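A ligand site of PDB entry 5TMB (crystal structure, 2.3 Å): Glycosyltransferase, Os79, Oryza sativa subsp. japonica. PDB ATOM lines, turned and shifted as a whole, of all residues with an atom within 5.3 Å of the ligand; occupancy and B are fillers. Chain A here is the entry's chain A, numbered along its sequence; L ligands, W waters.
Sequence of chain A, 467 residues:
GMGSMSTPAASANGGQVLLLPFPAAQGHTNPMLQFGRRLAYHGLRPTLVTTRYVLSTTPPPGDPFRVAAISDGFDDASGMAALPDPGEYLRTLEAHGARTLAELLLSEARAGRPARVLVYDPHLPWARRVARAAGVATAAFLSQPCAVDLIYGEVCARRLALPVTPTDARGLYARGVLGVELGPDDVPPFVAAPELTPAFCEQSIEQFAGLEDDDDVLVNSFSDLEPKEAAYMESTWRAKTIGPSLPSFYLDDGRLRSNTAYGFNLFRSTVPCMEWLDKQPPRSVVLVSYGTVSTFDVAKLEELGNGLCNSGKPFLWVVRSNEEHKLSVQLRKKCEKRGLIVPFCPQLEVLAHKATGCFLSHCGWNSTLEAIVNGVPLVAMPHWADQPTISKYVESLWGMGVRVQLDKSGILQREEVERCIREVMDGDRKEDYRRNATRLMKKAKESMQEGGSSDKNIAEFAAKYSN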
ATOM      1  N   GLN A  26      25.053  21.859  10.783  1.00  0.00           N
ATOM      2  CA  GLN A  26      23.669  21.474  11.020  1.00  0.00           C
ATOM      3  C   GLN A  26      23.285  20.225  10.235  1.00  0.00           C
ATOM      4  O   GLN A  26      22.578  19.358  10.737  1.00  0.00           O
ATOM      5  CB  GLN A  26      22.723  22.609  10.643  1.00  0.00           C
ATOM      6  CG  GLN A  26      21.299  22.401  11.142  1.00  0.00           C
ATOM      7  CD  GLN A  26      21.170  22.710  12.620  1.00  0.00           C
ATOM      8  OE1 GLN A  26      20.968  23.864  13.015  1.00  0.00           O
ATOM      9  NE2 GLN A  26      21.292  21.675  13.459  1.00  0.00           N
ATOM     10  N   GLY A  27      23.791  20.124   9.014  1.00  0.00           N
ATOM     11  CA  GLY A  27      23.451  19.007   8.168  1.00  0.00           C
ATOM     12  C   GLY A  27      24.093  17.701   8.599  1.00  0.00           C
ATOM     13  O   GLY A  27      23.783  16.633   8.060  1.00  0.00           O
ATOM     14  N   ASN A  30      22.141  17.160  12.855  1.00  0.00           N
ATOM     15  CA  ASN A  30      20.751  16.713  12.923  1.00  0.00           C
ATOM     16  C   ASN A  30      20.574  15.184  12.731  1.00  0.00           C
ATOM     17  O   ASN A  30      19.979  14.539  13.579  1.00  0.00           O
ATOM     18  CB  ASN A  30      19.898  17.481  11.897  1.00  0.00           C
ATOM     19  CG  ASN A  30      19.461  18.838  12.415  1.00  0.00           C
ATOM     20  OD1 ASN A  30      19.661  19.149  13.597  1.00  0.00           O
ATOM     21  ND2 ASN A  30      18.850  19.648  11.550  1.00  0.00           N
ATOM     22  N   TYR A 262      14.042  18.426  15.463  1.00  0.00           N
ATOM     23  CA  TYR A 262      15.468  18.396  15.731  1.00  0.00           C
ATOM     24  C   TYR A 262      15.704  19.239  16.979  1.00  0.00           C
ATOM     25  O   TYR A 262      15.083  20.290  17.136  1.00  0.00           O
ATOM     26  CB  TYR A 262      16.277  18.956  14.575  1.00  0.00           C
ATOM     27  CG  TYR A 262      16.214  18.158  13.302  1.00  0.00           C
ATOM     28  CD1 TYR A 262      15.675  18.709  12.157  1.00  0.00           C
ATOM     29  CD2 TYR A 262      16.738  16.865  13.235  1.00  0.00           C
ATOM     30  CE1 TYR A 262      15.623  18.017  10.978  1.00  0.00           C
ATOM     31  CE2 TYR A 262      16.703  16.145  12.058  1.00  0.00           C
ATOM     32  CZ  TYR A 262      16.126  16.734  10.919  1.00  0.00           C
ATOM     33  OH  TYR A 262      16.086  16.065   9.719  1.00  0.00           O
ATOM     34  N   ASN A 265      19.236  23.118  17.028  1.00  0.00           N
ATOM     35  CA  ASN A 265      19.330  24.151  15.997  1.00  0.00           C
ATOM     36  C   ASN A 265      20.507  25.085  16.264  1.00  0.00           C
ATOM     37  O   ASN A 265      20.634  25.634  17.352  1.00  0.00           O
ATOM     38  CB  ASN A 265      18.029  24.940  15.898  1.00  0.00           C
ATOM     39  CG  ASN A 265      16.886  24.132  15.298  1.00  0.00           C
ATOM     40  OD1 ASN A 265      17.104  23.209  14.512  1.00  0.00           O
ATOM     41  ND2 ASN A 265      15.661  24.482  15.659  1.00  0.00           N
ATOM     42  N   SER A 289      14.978  27.813   0.100  1.00  0.00           N
ATOM     43  CA  SER A 289      16.134  27.748   1.008  1.00  0.00           C
ATOM     44  C   SER A 289      17.345  27.184   0.294  1.00  0.00           C
ATOM     45  O   SER A 289      17.242  26.215  -0.450  1.00  0.00           O
ATOM     46  CB  SER A 289      15.812  26.883   2.222  1.00  0.00           C
ATOM     47  OG  SER A 289      16.916  26.825   3.105  1.00  0.00           O
ATOM     48  N   TYR A 290      18.509  27.773   0.509  1.00  0.00           N
ATOM     49  CA  TYR A 290      19.706  27.112   0.015  1.00  0.00           C
ATOM     50  C   TYR A 290      20.562  26.641   1.214  1.00  0.00           C
ATOM     51  O   TYR A 290      21.768  26.480   1.120  1.00  0.00           O
ATOM     52  CB  TYR A 290      20.488  28.025  -0.937  1.00  0.00           C
ATOM     53  CG  TYR A 290      20.714  29.418  -0.455  1.00  0.00           C
ATOM     54  CD1 TYR A 290      21.802  29.715   0.356  1.00  0.00           C
ATOM     55  CD2 TYR A 290      19.869  30.456  -0.813  1.00  0.00           C
ATOM     56  CE1 TYR A 290      22.034  31.006   0.818  1.00  0.00           C
ATOM     57  CE2 TYR A 290      20.086  31.754  -0.364  1.00  0.00           C
ATOM     58  CZ  TYR A 290      21.184  32.020   0.461  1.00  0.00           C
ATOM     59  OH  TYR A 290      21.425  33.288   0.923  1.00  0.00           O
ATOM     60  N   GLY A 291      19.897  26.392   2.335  1.00  0.00           N
ATOM     61  CA  GLY A 291      20.503  25.701   3.465  1.00  0.00           C
ATOM     62  C   GLY A 291      21.227  26.619   4.422  1.00  0.00           C
ATOM     63  O   GLY A 291      20.984  27.832   4.473  1.00  0.00           O
ATOM     64  N   THR A 292      22.128  26.029   5.190  1.00  0.00           N
ATOM     65  CA  THR A 292      22.779  26.729   6.304  1.00  0.00           C
ATOM     66  C   THR A 292      24.274  26.972   6.073  1.00  0.00           C
ATOM     67  O   THR A 292      24.950  27.503   6.944  1.00  0.00           O
ATOM     68  CB  THR A 292      22.608  25.935   7.624  1.00  0.00           C
ATOM     69  OG1 THR A 292      23.362  24.704   7.556  1.00  0.00           O
ATOM     70  CG2 THR A 292      21.135  25.611   7.880  1.00  0.00           C
ATOM     71  N   VAL A 293      24.797  26.595   4.910  1.00  0.00           N
ATOM     72  CA  VAL A 293      26.238  26.696   4.668  1.00  0.00           C
ATOM     73  C   VAL A 293      26.544  27.597   3.471  1.00  0.00           C
ATOM     74  O   VAL A 293      27.363  28.515   3.558  1.00  0.00           O
ATOM     75  CB  VAL A 293      26.842  25.306   4.402  1.00  0.00           C
ATOM     76  CG1 VAL A 293      28.373  25.394   4.218  1.00  0.00           C
ATOM     77  CG2 VAL A 293      26.466  24.336   5.533  1.00  0.00           C
ATOM     78  N   SER A 294      25.854  27.341   2.366  1.00  0.00           N
ATOM     79  CA  SER A 294      26.039  28.128   1.148  1.00  0.00           C
ATOM     80  C   SER A 294      25.736  29.614   1.351  1.00  0.00           C
ATOM     81  O   SER A 294      24.946  29.991   2.214  1.00  0.00           O
ATOM     82  CB  SER A 294      25.170  27.577   0.017  1.00  0.00           C
ATOM     83  OG  SER A 294      25.661  26.355  -0.509  1.00  0.00           O
ATOM     84  N   VAL A 318      13.515  31.567   3.044  1.00  0.00           N
ATOM     85  CA  VAL A 318      14.524  31.589   4.092  1.00  0.00           C
ATOM     86  C   VAL A 318      15.791  32.322   3.635  1.00  0.00           C
ATOM     87  O   VAL A 318      16.576  31.795   2.840  1.00  0.00           O
ATOM     88  CB  VAL A 318      14.934  30.171   4.536  1.00  0.00           C
ATOM     89  CG1 VAL A 318      15.877  30.258   5.743  1.00  0.00           C
ATOM     90  CG2 VAL A 318      13.701  29.355   4.887  1.00  0.00           C
ATOM     91  N   PRO A 343      14.637  34.451   8.799  1.00  0.00           N
ATOM     92  CA  PRO A 343      16.033  34.001   8.885  1.00  0.00           C
ATOM     93  C   PRO A 343      16.163  32.487   9.073  1.00  0.00           C
ATOM     94  O   PRO A 343      17.190  31.931   8.713  1.00  0.00           O
ATOM     95  CB  PRO A 343      16.573  34.759  10.118  1.00  0.00           C
ATOM     96  CG  PRO A 343      15.359  35.131  10.908  1.00  0.00           C
ATOM     97  CD  PRO A 343      14.252  35.332   9.927  1.00  0.00           C
ATOM     98  N   PHE A 344      15.160  31.837   9.639  1.00  0.00           N
ATOM     99  CA  PHE A 344      15.202  30.385   9.845  1.00  0.00           C
ATOM    100  C   PHE A 344      13.755  29.938   9.926  1.00  0.00           C
ATOM    101  O   PHE A 344      12.899  30.715  10.324  1.00  0.00           O
ATOM    102  CB  PHE A 344      15.984  30.018  11.120  1.00  0.00           C
ATOM    103  CG  PHE A 344      16.664  28.648  11.072  1.00  0.00           C
ATOM    104  CD1 PHE A 344      17.642  28.363  10.130  1.00  0.00           C
ATOM    105  CD2 PHE A 344      16.354  27.685  12.012  1.00  0.00           C
ATOM    106  CE1 PHE A 344      18.278  27.129  10.099  1.00  0.00           C
ATOM    107  CE2 PHE A 344      16.977  26.441  11.997  1.00  0.00           C
ATOM    108  CZ  PHE A 344      17.954  26.164  11.040  1.00  0.00           C
ATOM    109  N   CYS A 345      13.460  28.703   9.549  1.00  0.00           N
ATOM    110  CA  CYS A 345      12.116  28.221   9.752  1.00  0.00           C
ATOM    111  C   CYS A 345      12.162  26.793  10.288  1.00  0.00           C
ATOM    112  O   CYS A 345      13.169  26.104  10.121  1.00  0.00           O
ATOM    113  CB  CYS A 345      11.311  28.296   8.457  1.00  0.00           C
ATOM    114  SG  CYS A 345      11.750  27.018   7.266  1.00  0.00           S
ATOM    115  N   PRO A 346      11.079  26.357  10.968  1.00  0.00           N
ATOM    116  CA  PRO A 346      10.971  24.930  11.299  1.00  0.00           C
ATOM    117  C   PRO A 346      10.678  24.150  10.014  1.00  0.00           C
ATOM    118  O   PRO A 346       9.505  23.881   9.698  1.00  0.00           O
ATOM    119  CB  PRO A 346       9.807  24.893  12.295  1.00  0.00           C
ATOM    120  CG  PRO A 346       8.947  26.064  11.855  1.00  0.00           C
ATOM    121  CD  PRO A 346       9.890  27.125  11.369  1.00  0.00           C
ATOM    122  N   GLN A 347      11.742  23.829   9.283  1.00  0.00           N
ATOM    123  CA  GLN A 347      11.637  23.404   7.897  1.00  0.00           C
ATOM    124  C   GLN A 347      10.810  22.133   7.717  1.00  0.00           C
ATOM    125  O   GLN A 347      10.027  22.032   6.787  1.00  0.00           O
ATOM    126  CB  GLN A 347      13.045  23.240   7.282  1.00  0.00           C
ATOM    127  CG  GLN A 347      13.136  22.374   6.013  1.00  0.00           C
ATOM    128  CD  GLN A 347      14.378  22.657   5.200  1.00  0.00           C
ATOM    129  OE1 GLN A 347      14.837  23.801   5.130  1.00  0.00           O
ATOM    130  NE2 GLN A 347      14.941  21.632   4.594  1.00  0.00           N
ATOM    131  N   LEU A 348      10.959  21.180   8.628  1.00  0.00           N
ATOM    132  CA  LEU A 348      10.169  19.963   8.544  1.00  0.00           C
ATOM    133  C   LEU A 348       8.700  20.258   8.805  1.00  0.00           C
ATOM    134  O   LEU A 348       7.817  19.706   8.125  1.00  0.00           O
ATOM    135  CB  LEU A 348      10.686  18.915   9.541  1.00  0.00           C
ATOM    136  CG  LEU A 348      11.564  17.832   8.908  1.00  0.00           C
ATOM    137  CD1 LEU A 348      12.294  17.021   9.968  1.00  0.00           C
ATOM    138  CD2 LEU A 348      10.755  16.933   7.977  1.00  0.00           C
ATOM    139  N   HIS A 362      18.430  23.899  -2.456  1.00  0.00           N
ATOM    140  CA  HIS A 362      19.772  23.650  -2.986  1.00  0.00           C
ATOM    141  C   HIS A 362      20.045  22.141  -3.025  1.00  0.00           C
ATOM    142  O   HIS A 362      21.037  21.690  -3.596  1.00  0.00           O
ATOM    143  CB  HIS A 362      20.823  24.365  -2.155  1.00  0.00           C
ATOM    144  CG  HIS A 362      21.030  23.771  -0.805  1.00  0.00           C
ATOM    145  ND1 HIS A 362      19.983  23.470   0.043  1.00  0.00           N
ATOM    146  CD2 HIS A 362      22.163  23.418  -0.151  1.00  0.00           C
ATOM    147  CE1 HIS A 362      20.461  22.945   1.157  1.00  0.00           C
ATOM    148  NE2 HIS A 362      21.780  22.901   1.072  1.00  0.00           N
ATOM    149  N   GLY A 364      20.728  20.032  -0.497  1.00  0.00           N
ATOM    150  CA  GLY A 364      21.469  19.369   0.562  1.00  0.00           C
ATOM    151  C   GLY A 364      20.697  18.111   0.935  1.00  0.00           C
ATOM    152  O   GLY A 364      19.471  18.021   0.770  1.00  0.00           O
ATOM    153  N   TRP A 365      21.407  17.111   1.444  1.00  0.00           N
ATOM    154  CA  TRP A 365      20.801  15.808   1.591  1.00  0.00           C
ATOM    155  C   TRP A 365      19.682  15.807   2.657  1.00  0.00           C
ATOM    156  O   TRP A 365      18.659  15.157   2.465  1.00  0.00           O
ATOM    157  CB  TRP A 365      21.898  14.789   1.900  1.00  0.00           C
ATOM    158  CG  TRP A 365      21.478  13.373   1.928  1.00  0.00           C
ATOM    159  CD1 TRP A 365      21.764  12.460   2.915  1.00  0.00           C
ATOM    160  CD2 TRP A 365      20.715  12.660   0.933  1.00  0.00           C
ATOM    161  NE1 TRP A 365      21.230  11.219   2.581  1.00  0.00           N
ATOM    162  CE2 TRP A 365      20.572  11.320   1.380  1.00  0.00           C
ATOM    163  CE3 TRP A 365      20.143  13.018  -0.288  1.00  0.00           C
ATOM    164  CZ2 TRP A 365      19.894  10.359   0.660  1.00  0.00           C
ATOM    165  CZ3 TRP A 365      19.458  12.062  -1.010  1.00  0.00           C
ATOM    166  CH2 TRP A 365      19.344  10.737  -0.538  1.00  0.00           C
ATOM    167  N   ASN A 366      19.861  16.533   3.761  1.00  0.00           N
ATOM    168  CA  ASN A 366      18.788  16.535   4.769  1.00  0.00           C
ATOM    169  C   ASN A 366      17.510  17.188   4.192  1.00  0.00           C
ATOM    170  O   ASN A 366      16.429  16.622   4.305  1.00  0.00           O
ATOM    171  CB  ASN A 366      19.224  17.211   6.053  1.00  0.00           C
ATOM    172  CG  ASN A 366      20.467  16.574   6.657  1.00  0.00           C
ATOM    173  OD1 ASN A 366      20.431  15.440   7.139  1.00  0.00           O
ATOM    174  ND2 ASN A 366      21.568  17.298   6.615  1.00  0.00           N
ATOM    175  N   SER A 367      17.669  18.324   3.530  1.00  0.00           N
ATOM    176  CA  SER A 367      16.534  19.004   2.893  1.00  0.00           C
ATOM    177  C   SER A 367      15.817  18.072   1.920  1.00  0.00           C
ATOM    178  O   SER A 367      14.592  18.011   1.907  1.00  0.00           O
ATOM    179  CB  SER A 367      17.007  20.270   2.174  1.00  0.00           C
ATOM    180  OG  SER A 367      17.421  21.236   3.119  1.00  0.00           O
ATOM    181  N   THR A 368      16.593  17.304   1.147  1.00  0.00           N
ATOM    182  CA  THR A 368      15.998  16.374   0.202  1.00  0.00           C
ATOM    183  C   THR A 368      15.214  15.274   0.910  1.00  0.00           C
ATOM    184  O   THR A 368      14.062  14.971   0.532  1.00  0.00           O
ATOM    185  CB  THR A 368      17.072  15.766  -0.719  1.00  0.00           C
ATOM    186  OG1 THR A 368      17.815  16.813  -1.347  1.00  0.00           O
ATOM    187  CG2 THR A 368      16.441  14.915  -1.808  1.00  0.00           C
ATOM    188  N   GLU A 370      13.964  15.412   3.784  1.00  0.00           N
ATOM    189  CA  GLU A 370      12.855  16.020   4.485  1.00  0.00           C
ATOM    190  C   GLU A 370      11.673  16.279   3.513  1.00  0.00           C
ATOM    191  O   GLU A 370      10.514  16.145   3.893  1.00  0.00           O
ATOM    192  CB  GLU A 370      13.309  17.290   5.181  1.00  0.00           C
ATOM    193  CG  GLU A 370      14.160  17.013   6.413  1.00  0.00           C
ATOM    194  CD  GLU A 370      14.941  18.223   6.918  1.00  0.00           C
ATOM    195  OE1 GLU A 370      14.775  19.352   6.401  1.00  0.00           O
ATOM    196  OE2 GLU A 370      15.745  18.031   7.849  1.00  0.00           O
ATOM    197  N   GLN A 387      25.105  17.978  -3.802  1.00  0.00           N
ATOM    198  CA  GLN A 387      23.875  18.595  -4.331  1.00  0.00           C
ATOM    199  C   GLN A 387      23.663  18.354  -5.841  1.00  0.00           C
ATOM    200  O   GLN A 387      22.559  17.973  -6.229  1.00  0.00           O
ATOM    201  CB  GLN A 387      23.878  20.088  -4.009  1.00  0.00           C
ATOM    202  CG  GLN A 387      23.988  20.369  -2.492  1.00  0.00           C
ATOM    203  CD  GLN A 387      24.670  21.685  -2.197  1.00  0.00           C
ATOM    204  OE1 GLN A 387      24.815  22.519  -3.095  1.00  0.00           O
ATOM    205  NE2 GLN A 387      25.096  21.875  -0.955  1.00  0.00           N
HETATM  206  N1  LIG L   1      16.972  23.852   8.426  1.00  0.00           N
HETATM  207  C1  LIG L   1      15.997  24.325   9.284  1.00  0.00           C
HETATM  208  N2  LIG L   1      15.452  25.568   9.088  1.00  0.00           N
HETATM  209  C2  LIG L   1      15.868  26.353   8.039  1.00  0.00           C
HETATM  210  C3  LIG L   1      16.858  25.881   7.181  1.00  0.00           C
HETATM  211  C4  LIG L   1      17.534  24.722   7.532  1.00  0.00           C
HETATM  212  O1  LIG L   1      15.602  23.644  10.230  1.00  0.00           O
HETATM  213  O2  LIG L   1      15.379  27.462   7.881  1.00  0.00           O
HETATM  214  C5  LIG L   1      17.545  22.503   8.604  1.00  0.00           C
HETATM  215  C6  LIG L   1      16.923  21.570   7.573  1.00  0.00           C
HETATM  216  O3  LIG L   1      15.726  20.968   8.046  1.00  0.00           O
HETATM  217  C7  LIG L   1      18.013  20.549   7.323  1.00  0.00           C
HETATM  218  C8  LIG L   1      19.300  21.294   7.650  1.00  0.00           C
HETATM  219  O4  LIG L   1      18.930  22.469   8.336  1.00  0.00           O
HETATM  220  O5  LIG L   1      17.836  19.501   8.253  1.00  0.00           O
HETATM  221  C9  LIG L   1      20.097  21.664   6.404  1.00  0.00           C
HETATM  222  O6  LIG L   1      20.788  20.506   5.975  1.00  0.00           O
HETATM  223  P1  LIG L   1      21.074  20.198   4.415  1.00  0.00           P
HETATM  224  O7  LIG L   1      21.853  18.941   4.248  1.00  0.00           O
HETATM  225  O8  LIG L   1      19.823  20.043   3.644  1.00  0.00           O
HETATM  226  O9  LIG L   1      21.847  21.485   3.864  1.00  0.00           O
HETATM  227  P2  LIG L   1      23.186  22.144   4.470  1.00  0.00           P
HETATM  228  O10 LIG L   1      23.997  22.578   3.295  1.00  0.00           O
HETATM  229  O11 LIG L   1      22.787  23.326   5.265  1.00  0.00           O
HETATM  230  O12 LIG L   1      23.955  21.174   5.272  1.00  0.00           O
HETATM  231  O   HOH W   1      25.359  21.630   7.352  1.00  0.00           O
HETATM  232  O   HOH W   2      14.035  23.531  12.513  1.00  0.00           O
HETATM  233  O   HOH W   3      13.623  20.798   9.996  1.00  0.00           O
HETATM  234  O   HOH W   4      23.980  25.204   2.489  1.00  0.00           O
HETATM  235  O   HOH W   5      17.673  22.098  12.209  1.00  0.00           O
HETATM  236  O   HOH W   6      26.459  21.592   2.537  1.00  0.00           O
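An oxygen (O2) of the ligand lies within hydrogen-bond range of the backbone NH (N) of Cys 345 (2.8 Å). SG of Cys 345 lies within hydrogen-bond range of O2 of the ligand, 3.7 Å away. The backbone NH (N) of Trp 365 sits at hydrogen-bond distance from an oxygen (O7) of the ligand, 3.4 Å away. The side-chain carboxylate of Glu 370 is in hydrogen-bond range of an oxygen (O3) of the ligand. O7 of the ligand is in hydrogen-bond range of N of Asn 366 (3.2 Å). The backbone NH of Ser 367 lies within hydrogen-bond range of an oxygen (O8) of the ligand. An oxygen (O11) of the ligand lies within hydrogen-bond range of the backbone NH (N) of Thr 292 (2.8 Å). A ring nitrogen (NE2) of His 362 lies within hydrogen-bond range of an oxygen (O9) of the ligand, 3.1 Å away. OG1 of Thr 292 lies within hydrogen-bond range of O11 of the ligand, at 2.7 Å. O of Cys 345 sits at hydrogen-bond distance from N2 of the ligand (2.6 Å). The side-chain amide nitrogen (ND2) of Asn 30 sits at hydrogen-bond distance from an oxygen (O5) of the ligand (3.5 Å). OG of Ser 367 is in hydrogen-bond range of O8 of the ligand. The side-chain amide nitrogen (ND2) of Asn 366 sits at hydrogen-bond distance from an oxygen (O7) of the ligand (2.9 Å).
Water W1 lies within hydrogen-bond range of an oxygen (O12) of the ligand (2.6 Å), the backbone NH (N) of Gly 27 (2.7 Å) and the backbone NH (N) of Gln 26 (3.5 Å). Water W3 lies within hydrogen-bond range of O3 of the ligand and N of Leu 348. Water W5 lies within hydrogen-bond range of OD1 of Asn 265 (2.6 Å), ND2 of Asn 30 (2.8 Å) and O1 of the ligand (3.3 Å).
The side-chain hydroxyl of Ser 367 lies within hydrogen-bond range of the side-chain amide nitrogen of Gln 347, 2.9 Å away. OD1 of Asn 30 is in hydrogen-bond range of NE2 of Gln 26. The backbone carbonyl oxygen (O) of Gly 27 sits at hydrogen-bond distance from the side-chain amide nitrogen (ND2) of Asn 366 (2.7 Å). The backbone carbonyl oxygen (O) of Ser 289 lies within hydrogen-bond range of the backbone NH (N) of His 362 (3.3 Å). OE2 of Glu 370 lies within hydrogen-bond range of OH of Tyr 262 (2.7 Å). The side-chain sulfur (SG) of Cys 345 lies close to the backbone NH (N) of Gln 347 (3.8 Å). The backbone NH (N) of Gly 364 sits close to a ring nitrogen (NE2) of His 362. The side-chain carboxylate of Glu 370 sits at hydrogen-bond distance from the side-chain amide nitrogen of Gln 347 (2.9 Å).
Merely in contact with the ligand: Gln 26 (3.7 Å), Gly 27 (3.7 Å), Tyr 262 (3.8 Å), Gly 291 (3.7 Å), Val 293 (3.8 Å), Val 318 (3.6 Å), Phe 344 (3.2 Å), Gln 347 (3.6 Å) and Gly 364 (3.4 Å). Hydrophobic or aromatic side chains that line the ligand: Tyr 262, Val 293, Val 318, Phe 344 and His 362. Along chain A the residues within 4 Å of the ligand span positions 26 to 370. The nearest printed residue that does not touch the ligand is Ser 289 (4.2 Å).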
